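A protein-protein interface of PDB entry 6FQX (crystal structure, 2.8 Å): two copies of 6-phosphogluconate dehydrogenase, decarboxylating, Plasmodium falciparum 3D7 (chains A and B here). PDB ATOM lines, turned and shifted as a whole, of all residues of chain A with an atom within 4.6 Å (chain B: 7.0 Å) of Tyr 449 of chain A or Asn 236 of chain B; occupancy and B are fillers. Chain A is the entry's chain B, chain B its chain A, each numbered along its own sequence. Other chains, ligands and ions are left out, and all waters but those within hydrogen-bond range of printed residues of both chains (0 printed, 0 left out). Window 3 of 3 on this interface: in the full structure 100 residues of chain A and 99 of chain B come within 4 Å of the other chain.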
ATOM      1  N   ALA A 445      15.420  14.411  -9.743  1.00  0.00           N
ATOM      2  CA  ALA A 445      14.338  15.317 -10.132  1.00  0.00           C
ATOM      3  C   ALA A 445      13.531  15.773  -8.920  1.00  0.00           C
ATOM      4  O   ALA A 445      13.184  16.959  -8.813  1.00  0.00           O
ATOM      5  CB  ALA A 445      13.430  14.656 -11.170  1.00  0.00           C
ATOM      6  N   GLN A 446      13.220  14.860  -7.992  1.00  0.00           N
ATOM      7  CA  GLN A 446      12.501  15.306  -6.805  1.00  0.00           C
ATOM      8  C   GLN A 446      13.329  16.313  -6.035  1.00  0.00           C
ATOM      9  O   GLN A 446      12.824  17.370  -5.641  1.00  0.00           O
ATOM     10  CB  GLN A 446      12.137  14.135  -5.896  1.00  0.00           C
ATOM     11  CG  GLN A 446      11.197  13.160  -6.520  1.00  0.00           C
ATOM     12  CD  GLN A 446      11.293  11.786  -5.911  1.00  0.00           C
ATOM     13  OE1 GLN A 446      12.336  11.402  -5.415  1.00  0.00           O
ATOM     14  NE2 GLN A 446      10.196  11.021  -5.967  1.00  0.00           N
ATOM     15  N   ARG A 447      14.631  16.059  -5.912  1.00  0.00           N
ATOM     16  CA  ARG A 447      15.456  16.951  -5.113  1.00  0.00           C
ATOM     17  C   ARG A 447      15.537  18.336  -5.726  1.00  0.00           C
ATOM     18  O   ARG A 447      15.554  19.338  -4.999  1.00  0.00           O
ATOM     19  CB  ARG A 447      16.857  16.382  -4.965  1.00  0.00           C
ATOM     20  CG  ARG A 447      16.961  15.147  -4.147  1.00  0.00           C
ATOM     21  CD  ARG A 447      18.426  14.768  -4.030  1.00  0.00           C
ATOM     22  NE  ARG A 447      19.181  15.792  -3.289  1.00  0.00           N
ATOM     23  CZ  ARG A 447      20.088  16.602  -3.824  1.00  0.00           C
ATOM     24  NH1 ARG A 447      20.385  16.525  -5.114  1.00  0.00           N
ATOM     25  NH2 ARG A 447      20.702  17.485  -3.059  1.00  0.00           N
ATOM     26  N   ASP A 448      15.575  18.406  -7.062  1.00  0.00           N
ATOM     27  CA  ASP A 448      15.549  19.690  -7.753  1.00  0.00           C
ATOM     28  C   ASP A 448      14.197  20.374  -7.615  1.00  0.00           C
ATOM     29  O   ASP A 448      14.144  21.606  -7.501  1.00  0.00           O
ATOM     30  CB  ASP A 448      15.915  19.495  -9.225  1.00  0.00           C
ATOM     31  CG  ASP A 448      16.117  20.816  -9.964  1.00  0.00           C
ATOM     32  OD1 ASP A 448      17.041  21.595  -9.615  1.00  0.00           O
ATOM     33  OD2 ASP A 448      15.347  21.073 -10.916  1.00  0.00           O
ATOM     34  N   TYR A 449      13.107  19.589  -7.577  1.00  0.00           N
ATOM     35  CA  TYR A 449      11.764  20.148  -7.434  1.00  0.00           C
ATOM     36  C   TYR A 449      11.634  20.956  -6.142  1.00  0.00           C
ATOM     37  O   TYR A 449      11.206  22.110  -6.171  1.00  0.00           O
ATOM     38  CB  TYR A 449      10.720  19.024  -7.471  1.00  0.00           C
ATOM     39  CG  TYR A 449       9.269  19.483  -7.679  1.00  0.00           C
ATOM     40  CD1 TYR A 449       8.567  20.170  -6.677  1.00  0.00           C
ATOM     41  CD2 TYR A 449       8.582  19.179  -8.863  1.00  0.00           C
ATOM     42  CE1 TYR A 449       7.243  20.573  -6.866  1.00  0.00           C
ATOM     43  CE2 TYR A 449       7.259  19.574  -9.055  1.00  0.00           C
ATOM     44  CZ  TYR A 449       6.596  20.265  -8.056  1.00  0.00           C
ATOM     45  OH  TYR A 449       5.278  20.649  -8.260  1.00  0.00           O
ATOM     46  N   PHE A 450      11.970  20.362  -4.993  1.00  0.00           N
ATOM     47  CA  PHE A 450      11.726  21.046  -3.728  1.00  0.00           C
ATOM     48  C   PHE A 450      12.930  21.803  -3.168  1.00  0.00           C
ATOM     49  O   PHE A 450      12.742  22.710  -2.347  1.00  0.00           O
ATOM     50  CB  PHE A 450      11.218  20.059  -2.662  1.00  0.00           C
ATOM     51  CG  PHE A 450      12.150  18.902  -2.361  1.00  0.00           C
ATOM     52  CD1 PHE A 450      13.325  19.094  -1.644  1.00  0.00           C
ATOM     53  CD2 PHE A 450      11.820  17.609  -2.740  1.00  0.00           C
ATOM     54  CE1 PHE A 450      14.171  18.022  -1.343  1.00  0.00           C
ATOM     55  CE2 PHE A 450      12.667  16.537  -2.446  1.00  0.00           C
ATOM     56  CZ  PHE A 450      13.843  16.747  -1.748  1.00  0.00           C
ATOM     57  N   GLY A 451      14.148  21.476  -3.590  1.00  0.00           N
ATOM     58  CA  GLY A 451      15.320  22.094  -3.003  1.00  0.00           C
ATOM     59  C   GLY A 451      16.162  22.907  -3.963  1.00  0.00           C
ATOM     60  O   GLY A 451      17.102  23.596  -3.544  1.00  0.00           O
ATOM     61  N   TRP A 468       9.308  23.132 -12.430  1.00  0.00           N
ATOM     62  CA  TRP A 468       8.407  22.042 -12.731  1.00  0.00           C
ATOM     63  C   TRP A 468       6.984  22.570 -12.610  1.00  0.00           C
ATOM     64  O   TRP A 468       6.083  22.106 -13.323  1.00  0.00           O
ATOM     65  CB  TRP A 468       8.684  20.849 -11.808  1.00  0.00           C
ATOM     66  CG  TRP A 468      10.148  20.471 -11.785  1.00  0.00           C
ATOM     67  CD1 TRP A 468      11.151  21.097 -11.091  1.00  0.00           C
ATOM     68  CD2 TRP A 468      10.771  19.403 -12.512  1.00  0.00           C
ATOM     69  NE1 TRP A 468      12.354  20.480 -11.334  1.00  0.00           N
ATOM     70  CE2 TRP A 468      12.151  19.436 -12.202  1.00  0.00           C
ATOM     71  CE3 TRP A 468      10.298  18.414 -13.388  1.00  0.00           C
ATOM     72  CZ2 TRP A 468      13.064  18.515 -12.744  1.00  0.00           C
ATOM     73  CZ3 TRP A 468      11.202  17.503 -13.922  1.00  0.00           C
ATOM     74  CH2 TRP A 468      12.570  17.564 -13.601  1.00  0.00           C
ATOM     75  OXT TRP A 468       6.738  23.491 -11.810  1.00  0.00           O
ATOM     76  N   GLU B 131      12.102  26.099  -0.766  1.00  0.00           N
ATOM     77  CA  GLU B 131      11.930  27.531  -0.960  1.00  0.00           C
ATOM     78  C   GLU B 131      10.461  27.919  -0.881  1.00  0.00           C
ATOM     79  O   GLU B 131      10.128  28.990  -0.351  1.00  0.00           O
ATOM     80  CB  GLU B 131      12.492  27.945  -2.316  1.00  0.00           C
ATOM     81  CG  GLU B 131      13.816  27.308  -2.691  1.00  0.00           C
ATOM     82  CD  GLU B 131      14.342  27.811  -4.038  1.00  0.00           C
ATOM     83  OE1 GLU B 131      15.564  27.702  -4.280  1.00  0.00           O
ATOM     84  OE2 GLU B 131      13.526  28.265  -4.880  1.00  0.00           O
ATOM     85  N   ALA B 132       9.572  27.043  -1.365  1.00  0.00           N
ATOM     86  CA  ALA B 132       8.145  27.328  -1.308  1.00  0.00           C
ATOM     87  C   ALA B 132       7.639  27.378   0.129  1.00  0.00           C
ATOM     88  O   ALA B 132       6.906  28.304   0.501  1.00  0.00           O
ATOM     89  CB  ALA B 132       7.378  26.294  -2.120  1.00  0.00           C
ATOM     90  N   SER B 215       2.524   8.805 -14.642  1.00  0.00           N
ATOM     91  CA  SER B 215       2.092  10.036 -13.997  1.00  0.00           C
ATOM     92  C   SER B 215       0.611   9.988 -13.642  1.00  0.00           C
ATOM     93  O   SER B 215       0.198  10.511 -12.598  1.00  0.00           O
ATOM     94  CB  SER B 215       2.425  11.233 -14.884  1.00  0.00           C
ATOM     95  OG  SER B 215       1.320  11.617 -15.668  1.00  0.00           O
ATOM     96  N   PHE B 218       0.269   7.809 -10.440  1.00  0.00           N
ATOM     97  CA  PHE B 218       0.703   8.480  -9.212  1.00  0.00           C
ATOM     98  C   PHE B 218      -0.295   9.549  -8.764  1.00  0.00           C
ATOM     99  O   PHE B 218      -0.519   9.719  -7.555  1.00  0.00           O
ATOM    100  CB  PHE B 218       2.104   9.074  -9.385  1.00  0.00           C
ATOM    101  CG  PHE B 218       3.221   8.064  -9.197  1.00  0.00           C
ATOM    102  CD1 PHE B 218       3.562   7.602  -7.926  1.00  0.00           C
ATOM    103  CD2 PHE B 218       3.940   7.587 -10.280  1.00  0.00           C
ATOM    104  CE1 PHE B 218       4.584   6.684  -7.753  1.00  0.00           C
ATOM    105  CE2 PHE B 218       4.963   6.661 -10.104  1.00  0.00           C
ATOM    106  CZ  PHE B 218       5.280   6.213  -8.846  1.00  0.00           C
ATOM    107  N   ASN B 219      -0.931  10.263  -9.714  1.00  0.00           N
ATOM    108  CA  ASN B 219      -1.967  11.218  -9.318  1.00  0.00           C
ATOM    109  C   ASN B 219      -3.124  10.505  -8.649  1.00  0.00           C
ATOM    110  O   ASN B 219      -3.680  10.997  -7.664  1.00  0.00           O
ATOM    111  CB  ASN B 219      -2.515  12.005 -10.510  1.00  0.00           C
ATOM    112  CG  ASN B 219      -1.650  13.182 -10.900  1.00  0.00           C
ATOM    113  OD1 ASN B 219      -1.082  13.220 -11.989  1.00  0.00           O
ATOM    114  ND2 ASN B 219      -1.523  14.139  -9.993  1.00  0.00           N
ATOM    115  N   TYR B 229       3.107  14.920  -0.363  1.00  0.00           N
ATOM    116  CA  TYR B 229       3.772  15.902  -1.206  1.00  0.00           C
ATOM    117  C   TYR B 229       4.687  15.223  -2.216  1.00  0.00           C
ATOM    118  O   TYR B 229       4.737  15.638  -3.379  1.00  0.00           O
ATOM    119  CB  TYR B 229       4.513  16.932  -0.354  1.00  0.00           C
ATOM    120  CG  TYR B 229       5.371  17.873  -1.178  1.00  0.00           C
ATOM    121  CD1 TYR B 229       6.739  18.002  -0.924  1.00  0.00           C
ATOM    122  CD2 TYR B 229       4.816  18.680  -2.167  1.00  0.00           C
ATOM    123  CE1 TYR B 229       7.535  18.868  -1.664  1.00  0.00           C
ATOM    124  CE2 TYR B 229       5.607  19.546  -2.915  1.00  0.00           C
ATOM    125  CZ  TYR B 229       6.963  19.639  -2.658  1.00  0.00           C
ATOM    126  OH  TYR B 229       7.743  20.500  -3.391  1.00  0.00           O
ATOM    127  N   ILE B 231       4.478  12.142  -3.458  1.00  0.00           N
ATOM    128  CA  ILE B 231       3.739  11.399  -4.467  1.00  0.00           C
ATOM    129  C   ILE B 231       3.186  12.360  -5.514  1.00  0.00           C
ATOM    130  O   ILE B 231       3.185  12.051  -6.708  1.00  0.00           O
ATOM    131  CB  ILE B 231       2.638  10.549  -3.796  1.00  0.00           C
ATOM    132  CG1 ILE B 231       3.247   9.310  -3.122  1.00  0.00           C
ATOM    133  CG2 ILE B 231       1.561  10.113  -4.791  1.00  0.00           C
ATOM    134  CD1 ILE B 231       3.765   8.219  -4.075  1.00  0.00           C
ATOM    135  N   GLU B 232       2.772  13.560  -5.099  1.00  0.00           N
ATOM    136  CA  GLU B 232       2.255  14.554  -6.040  1.00  0.00           C
ATOM    137  C   GLU B 232       3.319  15.004  -7.044  1.00  0.00           C
ATOM    138  O   GLU B 232       3.037  15.117  -8.246  1.00  0.00           O
ATOM    139  CB  GLU B 232       1.731  15.776  -5.289  1.00  0.00           C
ATOM    140  CG  GLU B 232       1.229  16.859  -6.248  1.00  0.00           C
ATOM    141  CD  GLU B 232       0.748  18.117  -5.545  1.00  0.00           C
ATOM    142  OE1 GLU B 232       0.727  19.190  -6.196  1.00  0.00           O
ATOM    143  OE2 GLU B 232       0.331  18.005  -4.371  1.00  0.00           O
ATOM    144  N   ILE B 233       4.528  15.328  -6.571  1.00  0.00           N
ATOM    145  CA  ILE B 233       5.525  15.847  -7.497  1.00  0.00           C
ATOM    146  C   ILE B 233       6.047  14.743  -8.421  1.00  0.00           C
ATOM    147  O   ILE B 233       6.453  15.015  -9.557  1.00  0.00           O
ATOM    148  CB  ILE B 233       6.652  16.538  -6.718  1.00  0.00           C
ATOM    149  CG1 ILE B 233       7.544  15.505  -6.007  1.00  0.00           C
ATOM    150  CG2 ILE B 233       6.055  17.541  -5.729  1.00  0.00           C
ATOM    151  CD1 ILE B 233       8.808  16.087  -5.418  1.00  0.00           C
ATOM    152  N   THR B 234       6.007  13.482  -7.986  1.00  0.00           N
ATOM    153  CA  THR B 234       6.416  12.417  -8.894  1.00  0.00           C
ATOM    154  C   THR B 234       5.466  12.323 -10.071  1.00  0.00           C
ATOM    155  O   THR B 234       5.906  12.073 -11.202  1.00  0.00           O
ATOM    156  CB  THR B 234       6.506  11.072  -8.141  1.00  0.00           C
ATOM    157  OG1 THR B 234       7.072  11.270  -6.834  1.00  0.00           O
ATOM    158  CG2 THR B 234       7.287  10.006  -8.916  1.00  0.00           C
ATOM    159  N   ALA B 235       4.178  12.611  -9.838  1.00  0.00           N
ATOM    160  CA  ALA B 235       3.196  12.694 -10.917  1.00  0.00           C
ATOM    161  C   ALA B 235       3.525  13.838 -11.869  1.00  0.00           C
ATOM    162  O   ALA B 235       3.424  13.685 -13.093  1.00  0.00           O
ATOM    163  CB  ALA B 235       1.793  12.863 -10.326  1.00  0.00           C
ATOM    164  N   ASN B 236       3.901  14.998 -11.317  1.00  0.00           N
ATOM    165  CA  ASN B 236       4.322  16.127 -12.140  1.00  0.00           C
ATOM    166  C   ASN B 236       5.631  15.829 -12.862  1.00  0.00           C
ATOM    167  O   ASN B 236       5.750  16.071 -14.068  1.00  0.00           O
ATOM    168  CB  ASN B 236       4.480  17.379 -11.273  1.00  0.00           C
ATOM    169  CG  ASN B 236       3.200  17.769 -10.557  1.00  0.00           C
ATOM    170  OD1 ASN B 236       2.110  17.303 -10.917  1.00  0.00           O
ATOM    171  ND2 ASN B 236       3.320  18.635  -9.542  1.00  0.00           N
ATOM    172  N   ILE B 237       6.592  15.232 -12.153  1.00  0.00           N
ATOM    173  CA  ILE B 237       7.926  15.012 -12.707  1.00  0.00           C
ATOM    174  C   ILE B 237       7.865  14.045 -13.887  1.00  0.00           C
ATOM    175  O   ILE B 237       8.456  14.296 -14.944  1.00  0.00           O
ATOM    176  CB  ILE B 237       8.873  14.508 -11.597  1.00  0.00           C
ATOM    177  CG1 ILE B 237       9.246  15.657 -10.637  1.00  0.00           C
ATOM    178  CG2 ILE B 237      10.123  13.880 -12.199  1.00  0.00           C
ATOM    179  CD1 ILE B 237       9.783  15.235  -9.257  1.00  0.00           C
ATOM    180  N   LEU B 238       7.143  12.925 -13.728  1.00  0.00           N
ATOM    181  CA  LEU B 238       7.066  11.912 -14.787  1.00  0.00           C
ATOM    182  C   LEU B 238       6.239  12.369 -15.981  1.00  0.00           C
ATOM    183  O   LEU B 238       6.332  11.754 -17.049  1.00  0.00           O
ATOM    184  CB  LEU B 238       6.521  10.587 -14.251  1.00  0.00           C
ATOM    185  CG  LEU B 238       7.424   9.923 -13.205  1.00  0.00           C
ATOM    186  CD1 LEU B 238       6.700   8.828 -12.449  1.00  0.00           C
ATOM    187  CD2 LEU B 238       8.692   9.386 -13.839  1.00  0.00           C
ATOM    188  N   ALA B 239       5.432  13.421 -15.815  1.00  0.00           N
ATOM    189  CA  ALA B 239       4.685  14.026 -16.910  1.00  0.00           C
ATOM    190  C   ALA B 239       5.452  15.140 -17.628  1.00  0.00           C
ATOM    191  O   ALA B 239       5.191  15.371 -18.813  1.00  0.00           O
ATOM    192  CB  ALA B 239       3.358  14.587 -16.383  1.00  0.00           C
ATOM    193  N   LYS B 240       6.434  15.779 -16.973  1.00  0.00           N
ATOM    194  CA  LYS B 240       7.129  16.917 -17.569  1.00  0.00           C
ATOM    195  C   LYS B 240       7.870  16.486 -18.825  1.00  0.00           C
ATOM    196  O   LYS B 240       8.533  15.446 -18.845  1.00  0.00           O
ATOM    197  CB  LYS B 240       8.123  17.554 -16.597  1.00  0.00           C
ATOM    198  CG  LYS B 240       8.835  18.778 -17.203  1.00  0.00           C
ATOM    199  CD  LYS B 240       8.036  20.072 -17.044  1.00  0.00           C
ATOM    200  CE  LYS B 240       8.796  21.269 -17.611  1.00  0.00           C
ATOM    201  NZ  LYS B 240       8.074  22.558 -17.414  1.00  0.00           N
ATOM    202  N   LYS B 241       7.762  17.295 -19.873  1.00  0.00           N
ATOM    203  CA  LYS B 241       8.365  16.977 -21.155  1.00  0.00           C
ATOM    204  C   LYS B 241       9.586  17.892 -21.313  1.00  0.00           C
ATOM    205  O   LYS B 241       9.604  19.015 -20.798  1.00  0.00           O
ATOM    206  CB  LYS B 241       7.340  17.211 -22.291  1.00  0.00           C
ATOM    207  CG  LYS B 241       5.833  17.034 -21.795  1.00  0.00           C
ATOM    208  CD  LYS B 241       4.595  16.785 -22.764  1.00  0.00           C
ATOM    209  CE  LYS B 241       4.332  15.419 -23.321  1.00  0.00           C
ATOM    210  NZ  LYS B 241       2.850  15.530 -23.405  1.00  0.00           N
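No position is printed for both chains.
The side-chain hydroxyl (OG1) of Thr 234 of chain B sits at hydrogen-bond distance from the side-chain amide nitrogen (NE2) of Gln 446 of chain A, at 3.3 Å.
The side-chain amide nitrogen (ND2) of Asn 236 of chain B lies within hydrogen-bond range of the side-chain hydroxyl (OH) of Tyr 449 of chain A (3.1 Å).
The side-chain carboxylate (OD2) of Asp 448 of chain A is in hydrogen-bond range of the indole nitrogen (NE1) of Trp 468 of chain A (3.1 Å).
Printed residues of chain B that touch a printed residue of chain A: Glu 131, Tyr 229, Ile 233, Thr 234, Asn 236, Ile 237 and Lys 240.
Hydrophobic or aromatic side chains of chain B within 4 Å of the printed part of chain A: Tyr 229, Ile 233 and Ile 237.
Among the printed residues, no Asp or Glu carboxylate lies within 4 Å of a Lys or Arg side-chain nitrogen of the other chain.
CB of Ala 445 of chain A touches CG2 of Ile 237 of chain B, at 3.5 Å.
Gln 446 of chain A touches Ile 233 of chain B.
CD1 of Ile 237 of chain B touches CA of Gln 446 of chain A (3.7 Å).
CD1 of Tyr 449 of chain A touches OH of Tyr 229 of chain B, 3.4 Å away.
CG2 of Ile 233 of chain B touches CE1 of Tyr 449 of chain A, 3.4 Å away.
Tyr 449 of chain A touches Ile 237 of chain B.
O of Phe 450 of chain A touches N of Glu 131 of chain B, 3.8 Å away.
CB of Phe 450 of chain A touches OH of Tyr 229 of chain B, 3.6 Å away.
Trp 468 of chain A touches Lys 240 of chain B (CE3 to CB, 3.97 Å).
Of the printed residues of chain B, Ala 445 of chain A touches Ile 237.
Asp 448 of chain A touches none of the printed residues of chain B.
Of the printed residues of chain B, Tyr 449 of chain A touches Tyr 229 (3.4 Å), Ile 233 (3.4 Å), Asn 236 (3.1 Å) and Ile 237 (3.999 Å).
Of the printed residues of chain B, Trp 468 of chain A touches Lys 240.
Printed residues of chain A within 4 Å of Ile 233 of chain B: Gln 446 (3.9 Å) and Tyr 449 (3.4 Å).
Of the printed residues of chain A, Thr 234 of chain B touches Gln 446 (3.3 Å).
Asn 236 of chain B touches just one residue of chain A: Tyr 449 (3.1 Å).
Of the printed residues of chain A, Ile 237 of chain B touches Ala 445 (3.5 Å), Gln 446 (3.7 Å) and Tyr 449 (3.999 Å).
The nearest printed residue of chain A that does not touch Asn 236 of chain B is Trp 468 of chain A (5.2 Å).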
